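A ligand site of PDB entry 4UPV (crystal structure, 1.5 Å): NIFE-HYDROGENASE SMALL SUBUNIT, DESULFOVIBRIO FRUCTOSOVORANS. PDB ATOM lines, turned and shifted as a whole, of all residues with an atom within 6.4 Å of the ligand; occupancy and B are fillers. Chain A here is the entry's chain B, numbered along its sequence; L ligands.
A ring nitrogen (ND1) of His 185 binds an iron atom (FE3) of the ligand, at 2.1 Å. SG of Cys 213 is bound to FE1 of the ligand (2.3 Å). FE2 of the ligand is bound by SG of Cys 188. An iron atom (FE4) of the ligand is bound by the side-chain sulfur (SG) of Cys 219 (2.3 Å). The backbone NH of Leu 214 sits close to a sulfur (S3) of the ligand. The backbone NH of Leu 191 lies close to a sulfur (S4) of the ligand (3.6 Å).
O of Gly 221 is in hydrogen-bond range of N of His 185. N of Tyr 215 sits close to SG of Cys 213, 3.4 Å away. SG of Cys 188 lies close to N of Arg 190 (3.3 Å). The backbone NH (N) of Cys 219 lies within hydrogen-bond range of the backbone carbonyl oxygen (O) of Leu 214 (3.3 Å). The backbone NH of Gly 221 sits close to the side-chain sulfur of Cys 219, at 3.4 Å. The side-chain sulfur (SG) of Cys 219 lies close to the backbone NH (N) of Cys 246, 3.5 Å away. The backbone carbonyl oxygen (O) of Cys 219 lies within hydrogen-bond range of the side-chain amide nitrogen (NE2) of Gln 264 (3.0 Å). O of Phe 212 lies within hydrogen-bond range of NH1 of Arg 190, at 2.9 Å.
The backbone carbonyl oxygen of Arg 190 sits close to a sulfur (S4) of the ligand. Merely in contact with the ligand: Phe 194, Tyr 215, Gly 221, Pro 222 and Val 240. Hydrophobic or aromatic side chains that line the ligand: His 185, Phe 194, Leu 214, Tyr 215, Pro 222 and Val 240. Of the 24 residues printed, 12 come within 4 Å of the ligand.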
ATOM      1  N   VAL A 184      23.231  -0.169  -0.886  1.00  0.00           N
ATOM      2  CA  VAL A 184      24.476   0.193  -0.206  1.00  0.00           C
ATOM      3  C   VAL A 184      24.217   1.400   0.701  1.00  0.00           C
ATOM      4  O   VAL A 184      24.559   1.413   1.897  1.00  0.00           O
ATOM      5  CB  VAL A 184      25.587   0.488  -1.258  1.00  0.00           C
ATOM      6  CG1 VAL A 184      26.746   1.218  -0.600  1.00  0.00           C
ATOM      7  CG2 VAL A 184      26.078  -0.809  -1.943  1.00  0.00           C
ATOM      8  N   HIS A 185      23.558   2.409   0.125  1.00  0.00           N
ATOM      9  CA  HIS A 185      23.320   3.676   0.826  1.00  0.00           C
ATOM     10  C   HIS A 185      22.540   3.472   2.120  1.00  0.00           C
ATOM     11  O   HIS A 185      22.760   4.177   3.129  1.00  0.00           O
ATOM     12  CB  HIS A 185      22.555   4.537  -0.153  1.00  0.00           C
ATOM     13  CG  HIS A 185      22.078   5.843   0.384  1.00  0.00           C
ATOM     14  ND1 HIS A 185      22.922   6.921   0.598  1.00  0.00           N
ATOM     15  CD2 HIS A 185      20.828   6.279   0.658  1.00  0.00           C
ATOM     16  CE1 HIS A 185      22.194   7.967   0.978  1.00  0.00           C
ATOM     17  NE2 HIS A 185      20.926   7.596   1.018  1.00  0.00           N
ATOM     18  N   ASP A 186      21.560   2.570   2.095  1.00  0.00           N
ATOM     19  CA  ASP A 186      20.690   2.430   3.258  1.00  0.00           C
ATOM     20  C   ASP A 186      21.399   1.947   4.513  1.00  0.00           C
ATOM     21  O   ASP A 186      20.908   2.159   5.614  1.00  0.00           O
ATOM     22  CB  ASP A 186      19.435   1.627   2.919  1.00  0.00           C
ATOM     23  CG  ASP A 186      18.460   2.444   2.055  1.00  0.00           C
ATOM     24  OD1 ASP A 186      18.623   3.696   1.885  1.00  0.00           O
ATOM     25  OD2 ASP A 186      17.511   1.839   1.554  1.00  0.00           O
ATOM     26  N   CYS A 188      24.880   2.710   4.882  1.00  0.00           N
ATOM     27  CA  CYS A 188      26.147   3.440   4.911  1.00  0.00           C
ATOM     28  C   CYS A 188      26.275   4.252   6.204  1.00  0.00           C
ATOM     29  O   CYS A 188      25.360   4.987   6.553  1.00  0.00           O
ATOM     30  CB  CYS A 188      26.180   4.388   3.706  1.00  0.00           C
ATOM     31  SG  CYS A 188      27.737   5.298   3.673  1.00  0.00           S
ATOM     32  N   PRO A 189      27.431   4.150   6.898  1.00  0.00           N
ATOM     33  CA  PRO A 189      27.584   4.986   8.090  1.00  0.00           C
ATOM     34  C   PRO A 189      27.626   6.480   7.835  1.00  0.00           C
ATOM     35  O   PRO A 189      27.563   7.251   8.787  1.00  0.00           O
ATOM     36  CB  PRO A 189      28.923   4.517   8.693  1.00  0.00           C
ATOM     37  CG  PRO A 189      29.120   3.131   8.177  1.00  0.00           C
ATOM     38  CD  PRO A 189      28.515   3.171   6.775  1.00  0.00           C
ATOM     39  N   ARG A 190      27.736   6.900   6.564  1.00  0.00           N
ATOM     40  CA  ARG A 190      27.697   8.330   6.236  1.00  0.00           C
ATOM     41  C   ARG A 190      26.275   8.821   5.976  1.00  0.00           C
ATOM     42  O   ARG A 190      26.078  10.020   5.714  1.00  0.00           O
ATOM     43  CB  ARG A 190      28.617   8.651   5.061  1.00  0.00           C
ATOM     44  CG  ARG A 190      30.067   8.275   5.371  1.00  0.00           C
ATOM     45  CD  ARG A 190      31.062   8.843   4.388  1.00  0.00           C
ATOM     46  NE  ARG A 190      32.400   8.344   4.728  1.00  0.00           N
ATOM     47  CZ  ARG A 190      33.551   8.910   4.366  1.00  0.00           C
ATOM     48  NH1 ARG A 190      33.579  10.039   3.639  1.00  0.00           N
ATOM     49  NH2 ARG A 190      34.694   8.365   4.764  1.00  0.00           N
ATOM     50  N   LEU A 191      25.300   7.924   6.119  1.00  0.00           N
ATOM     51  CA  LEU A 191      23.904   8.303   5.876  1.00  0.00           C
ATOM     52  C   LEU A 191      23.424   9.517   6.694  1.00  0.00           C
ATOM     53  O   LEU A 191      22.730  10.379   6.157  1.00  0.00           O
ATOM     54  CB  LEU A 191      22.984   7.076   6.001  1.00  0.00           C
ATOM     55  CG  LEU A 191      21.508   7.324   5.660  1.00  0.00           C
ATOM     56  CD1 LEU A 191      21.332   7.689   4.182  1.00  0.00           C
ATOM     57  CD2 LEU A 191      20.692   6.086   6.011  1.00  0.00           C
ATOM     58  N   PRO A 192      23.815   9.620   7.991  1.00  0.00           N
ATOM     59  CA  PRO A 192      23.381  10.821   8.719  1.00  0.00           C
ATOM     60  C   PRO A 192      23.934  12.110   8.089  1.00  0.00           C
ATOM     61  O   PRO A 192      23.235  13.155   8.103  1.00  0.00           O
ATOM     62  CB  PRO A 192      23.940  10.598  10.140  1.00  0.00           C
ATOM     63  CG  PRO A 192      24.052   9.116  10.265  1.00  0.00           C
ATOM     64  CD  PRO A 192      24.417   8.604   8.898  1.00  0.00           C
ATOM     65  N   HIS A 193      25.142  12.060   7.510  1.00  0.00           N
ATOM     66  CA  HIS A 193      25.623  13.246   6.751  1.00  0.00           C
ATOM     67  C   HIS A 193      24.779  13.503   5.503  1.00  0.00           C
ATOM     68  O   HIS A 193      24.424  14.659   5.219  1.00  0.00           O
ATOM     69  CB  HIS A 193      27.091  13.126   6.360  1.00  0.00           C
ATOM     70  CG  HIS A 193      28.039  13.225   7.522  1.00  0.00           C
ATOM     71  ND1 HIS A 193      28.036  14.276   8.422  1.00  0.00           N
ATOM     72  CD2 HIS A 193      29.032  12.397   7.927  1.00  0.00           C
ATOM     73  CE1 HIS A 193      29.003  14.097   9.315  1.00  0.00           C
ATOM     74  NE2 HIS A 193      29.599  12.952   9.047  1.00  0.00           N
ATOM     75  N   PHE A 194      24.489  12.445   4.743  1.00  0.00           N
ATOM     76  CA  PHE A 194      23.653  12.608   3.564  1.00  0.00           C
ATOM     77  C   PHE A 194      22.316  13.289   3.915  1.00  0.00           C
ATOM     78  O   PHE A 194      21.909  14.262   3.269  1.00  0.00           O
ATOM     79  CB  PHE A 194      23.409  11.252   2.887  1.00  0.00           C
ATOM     80  CG  PHE A 194      22.440  11.310   1.733  1.00  0.00           C
ATOM     81  CD1 PHE A 194      22.896  11.579   0.441  1.00  0.00           C
ATOM     82  CD2 PHE A 194      21.079  11.045   1.925  1.00  0.00           C
ATOM     83  CE1 PHE A 194      22.008  11.631  -0.628  1.00  0.00           C
ATOM     84  CE2 PHE A 194      20.195  11.047   0.848  1.00  0.00           C
ATOM     85  CZ  PHE A 194      20.662  11.320  -0.437  1.00  0.00           C
ATOM     86  N   PHE A 199      28.164  17.205   2.641  1.00  0.00           N
ATOM     87  CA  PHE A 199      28.884  16.583   1.528  1.00  0.00           C
ATOM     88  C   PHE A 199      30.300  17.088   1.404  1.00  0.00           C
ATOM     89  O   PHE A 199      30.561  18.270   1.623  1.00  0.00           O
ATOM     90  CB  PHE A 199      28.172  16.891   0.211  1.00  0.00           C
ATOM     91  CG  PHE A 199      26.719  16.508   0.183  1.00  0.00           C
ATOM     92  CD1 PHE A 199      26.354  15.160   0.167  1.00  0.00           C
ATOM     93  CD2 PHE A 199      25.718  17.472   0.122  1.00  0.00           C
ATOM     94  CE1 PHE A 199      25.040  14.755   0.113  1.00  0.00           C
ATOM     95  CE2 PHE A 199      24.382  17.081   0.085  1.00  0.00           C
ATOM     96  CZ  PHE A 199      24.033  15.730   0.071  1.00  0.00           C
ATOM     97  N   PHE A 212      32.456  13.343   5.551  1.00  0.00           N
ATOM     98  CA  PHE A 212      31.151  13.756   4.993  1.00  0.00           C
ATOM     99  C   PHE A 212      30.761  12.854   3.828  1.00  0.00           C
ATOM    100  O   PHE A 212      31.587  12.091   3.278  1.00  0.00           O
ATOM    101  CB  PHE A 212      31.179  15.221   4.555  1.00  0.00           C
ATOM    102  CG  PHE A 212      31.009  16.240   5.694  1.00  0.00           C
ATOM    103  CD1 PHE A 212      31.230  15.898   7.034  1.00  0.00           C
ATOM    104  CD2 PHE A 212      30.612  17.551   5.380  1.00  0.00           C
ATOM    105  CE1 PHE A 212      31.063  16.869   8.046  1.00  0.00           C
ATOM    106  CE2 PHE A 212      30.443  18.505   6.375  1.00  0.00           C
ATOM    107  CZ  PHE A 212      30.686  18.180   7.697  1.00  0.00           C
ATOM    108  N   CYS A 213      29.476  12.884   3.493  1.00  0.00           N
ATOM    109  CA  CYS A 213      28.966  12.016   2.432  1.00  0.00           C
ATOM    110  C   CYS A 213      29.633  12.331   1.097  1.00  0.00           C
ATOM    111  O   CYS A 213      29.981  13.475   0.809  1.00  0.00           O
ATOM    112  CB  CYS A 213      27.435  12.211   2.368  1.00  0.00           C
ATOM    113  SG  CYS A 213      26.629  11.492   0.926  1.00  0.00           S
ATOM    114  N   LEU A 214      29.795  11.282   0.290  1.00  0.00           N
ATOM    115  CA  LEU A 214      30.526  11.345  -1.003  1.00  0.00           C
ATOM    116  C   LEU A 214      29.614  11.489  -2.230  1.00  0.00           C
ATOM    117  O   LEU A 214      30.043  11.301  -3.383  1.00  0.00           O
ATOM    118  CB  LEU A 214      31.360  10.059  -1.109  1.00  0.00           C
ATOM    119  CG  LEU A 214      32.372   9.908   0.035  1.00  0.00           C
ATOM    120  CD1 LEU A 214      33.106   8.573  -0.103  1.00  0.00           C
ATOM    121  CD2 LEU A 214      33.384  11.086   0.118  1.00  0.00           C
ATOM    122  N   TYR A 215      28.338  11.824  -2.002  1.00  0.00           N
ATOM    123  CA  TYR A 215      27.377  11.887  -3.099  1.00  0.00           C
ATOM    124  C   TYR A 215      27.773  12.905  -4.195  1.00  0.00           C
ATOM    125  O   TYR A 215      27.583  12.658  -5.380  1.00  0.00           O
ATOM    126  CB  TYR A 215      25.976  12.171  -2.589  1.00  0.00           C
ATOM    127  CG  TYR A 215      24.912  11.944  -3.624  1.00  0.00           C
ATOM    128  CD1 TYR A 215      24.456  10.657  -3.915  1.00  0.00           C
ATOM    129  CD2 TYR A 215      24.345  13.025  -4.297  1.00  0.00           C
ATOM    130  CE1 TYR A 215      23.458  10.463  -4.891  1.00  0.00           C
ATOM    131  CE2 TYR A 215      23.379  12.841  -5.275  1.00  0.00           C
ATOM    132  CZ  TYR A 215      22.941  11.564  -5.561  1.00  0.00           C
ATOM    133  OH  TYR A 215      21.963  11.351  -6.531  1.00  0.00           O
ATOM    134  N   CYS A 219      29.081   9.229  -5.720  1.00  0.00           N
ATOM    135  CA  CYS A 219      28.721   7.978  -5.065  1.00  0.00           C
ATOM    136  C   CYS A 219      27.435   7.383  -5.602  1.00  0.00           C
ATOM    137  O   CYS A 219      26.391   8.068  -5.595  1.00  0.00           O
ATOM    138  CB  CYS A 219      28.539   8.168  -3.545  1.00  0.00           C
ATOM    139  SG  CYS A 219      28.469   6.582  -2.694  1.00  0.00           S
ATOM    140  N   LYS A 220      27.509   6.126  -6.061  1.00  0.00           N
ATOM    141  CA  LYS A 220      26.334   5.410  -6.547  1.00  0.00           C
ATOM    142  C   LYS A 220      25.697   4.503  -5.504  1.00  0.00           C
ATOM    143  O   LYS A 220      24.770   3.770  -5.823  1.00  0.00           O
ATOM    144  CB  LYS A 220      26.707   4.618  -7.814  1.00  0.00           C
ATOM    145  CG  LYS A 220      27.355   5.496  -8.923  1.00  0.00           C
ATOM    146  CD  LYS A 220      26.421   6.669  -9.296  1.00  0.00           C
ATOM    147  CE  LYS A 220      26.890   7.474 -10.522  1.00  0.00           C
ATOM    148  NZ  LYS A 220      28.343   7.857 -10.494  1.00  0.00           N
ATOM    149  N   GLY A 221      26.071   4.662  -4.237  1.00  0.00           N
ATOM    150  CA  GLY A 221      25.449   3.879  -3.169  1.00  0.00           C
ATOM    151  C   GLY A 221      23.922   3.975  -3.198  1.00  0.00           C
ATOM    152  O   GLY A 221      23.247   2.964  -2.942  1.00  0.00           O
ATOM    153  N   PRO A 222      23.370   5.165  -3.469  1.00  0.00           N
ATOM    154  CA  PRO A 222      21.912   5.296  -3.477  1.00  0.00           C
ATOM    155  C   PRO A 222      21.144   4.549  -4.564  1.00  0.00           C
ATOM    156  O   PRO A 222      19.899   4.459  -4.483  1.00  0.00           O
ATOM    157  CB  PRO A 222      21.690   6.801  -3.625  1.00  0.00           C
ATOM    158  CG  PRO A 222      22.936   7.412  -3.013  1.00  0.00           C
ATOM    159  CD  PRO A 222      24.042   6.485  -3.443  1.00  0.00           C
ATOM    160  N   TRP A 238      35.549  -1.004   3.496  1.00  0.00           N
ATOM    161  CA  TRP A 238      34.822  -0.966   2.223  1.00  0.00           C
ATOM    162  C   TRP A 238      35.100   0.391   1.581  1.00  0.00           C
ATOM    163  O   TRP A 238      35.651   1.281   2.242  1.00  0.00           O
ATOM    164  CB  TRP A 238      33.333  -1.290   2.406  1.00  0.00           C
ATOM    165  CG  TRP A 238      32.512  -0.206   3.080  1.00  0.00           C
ATOM    166  CD1 TRP A 238      32.586   0.212   4.406  1.00  0.00           C
ATOM    167  CD2 TRP A 238      31.475   0.574   2.467  1.00  0.00           C
ATOM    168  NE1 TRP A 238      31.638   1.203   4.625  1.00  0.00           N
ATOM    169  CE2 TRP A 238      30.948   1.435   3.461  1.00  0.00           C
ATOM    170  CE3 TRP A 238      30.930   0.609   1.186  1.00  0.00           C
ATOM    171  CZ2 TRP A 238      29.907   2.350   3.200  1.00  0.00           C
ATOM    172  CZ3 TRP A 238      29.900   1.506   0.900  1.00  0.00           C
ATOM    173  CH2 TRP A 238      29.377   2.368   1.917  1.00  0.00           C
ATOM    174  N   VAL A 240      33.635   3.274   0.729  1.00  0.00           N
ATOM    175  CA  VAL A 240      33.276   4.547   1.344  1.00  0.00           C
ATOM    176  C   VAL A 240      34.050   4.790   2.644  1.00  0.00           C
ATOM    177  O   VAL A 240      34.429   5.940   2.942  1.00  0.00           O
ATOM    178  CB  VAL A 240      31.751   4.668   1.491  1.00  0.00           C
ATOM    179  CG1 VAL A 240      31.348   5.788   2.448  1.00  0.00           C
ATOM    180  CG2 VAL A 240      31.116   4.845   0.095  1.00  0.00           C
ATOM    181  N   PRO A 245      33.857   7.138  -3.406  1.00  0.00           N
ATOM    182  CA  PRO A 245      32.472   6.800  -3.745  1.00  0.00           C
ATOM    183  C   PRO A 245      32.315   5.370  -4.281  1.00  0.00           C
ATOM    184  O   PRO A 245      33.247   4.810  -4.817  1.00  0.00           O
ATOM    185  CB  PRO A 245      32.138   7.804  -4.867  1.00  0.00           C
ATOM    186  CG  PRO A 245      33.477   8.296  -5.386  1.00  0.00           C
ATOM    187  CD  PRO A 245      34.333   8.305  -4.144  1.00  0.00           C
ATOM    188  N   CYS A 246      31.136   4.812  -4.069  1.00  0.00           N
ATOM    189  CA  CYS A 246      30.700   3.577  -4.727  1.00  0.00           C
ATOM    190  C   CYS A 246      30.543   3.816  -6.213  1.00  0.00           C
ATOM    191  O   CYS A 246      30.037   4.858  -6.647  1.00  0.00           O
ATOM    192  CB  CYS A 246      29.374   3.147  -4.085  1.00  0.00           C
ATOM    193  SG  CYS A 246      28.550   1.712  -4.825  1.00  0.00           S
ATOM    194  N   GLN A 264      27.138  12.746 -10.913  1.00  0.00           N
ATOM    195  CA  GLN A 264      25.792  12.160 -10.881  1.00  0.00           C
ATOM    196  C   GLN A 264      25.148  12.316 -12.280  1.00  0.00           C
ATOM    197  O   GLN A 264      24.409  13.257 -12.509  1.00  0.00           O
ATOM    198  CB  GLN A 264      24.921  12.795  -9.763  1.00  0.00           C
ATOM    199  CG  GLN A 264      25.467  12.524  -8.351  1.00  0.00           C
ATOM    200  CD  GLN A 264      25.445  11.038  -7.973  1.00  0.00           C
ATOM    201  OE1 GLN A 264      24.726  10.220  -8.585  1.00  0.00           O
ATOM    202  NE2 GLN A 264      26.202  10.685  -6.950  1.00  0.00           N
HETATM  203 FE1  LIG L   1      26.717   9.225   1.008  1.00  0.00          FE
HETATM  204 FE2  LIG L   1      27.211   6.721   1.968  1.00  0.00          FE
HETATM  205 FE3  LIG L   1      24.991   7.212   0.509  1.00  0.00          FE
HETATM  206 FE4  LIG L   1      27.448   7.184  -0.720  1.00  0.00          FE
HETATM  207  S1  LIG L   1      26.371   5.406   0.234  1.00  0.00           S
HETATM  208  S2  LIG L   1      25.749   8.682  -1.037  1.00  0.00           S
HETATM  209  S3  LIG L   1      28.716   8.112   0.994  1.00  0.00           S
HETATM  210  S4  LIG L   1      25.513   8.131   2.570  1.00  0.00           S
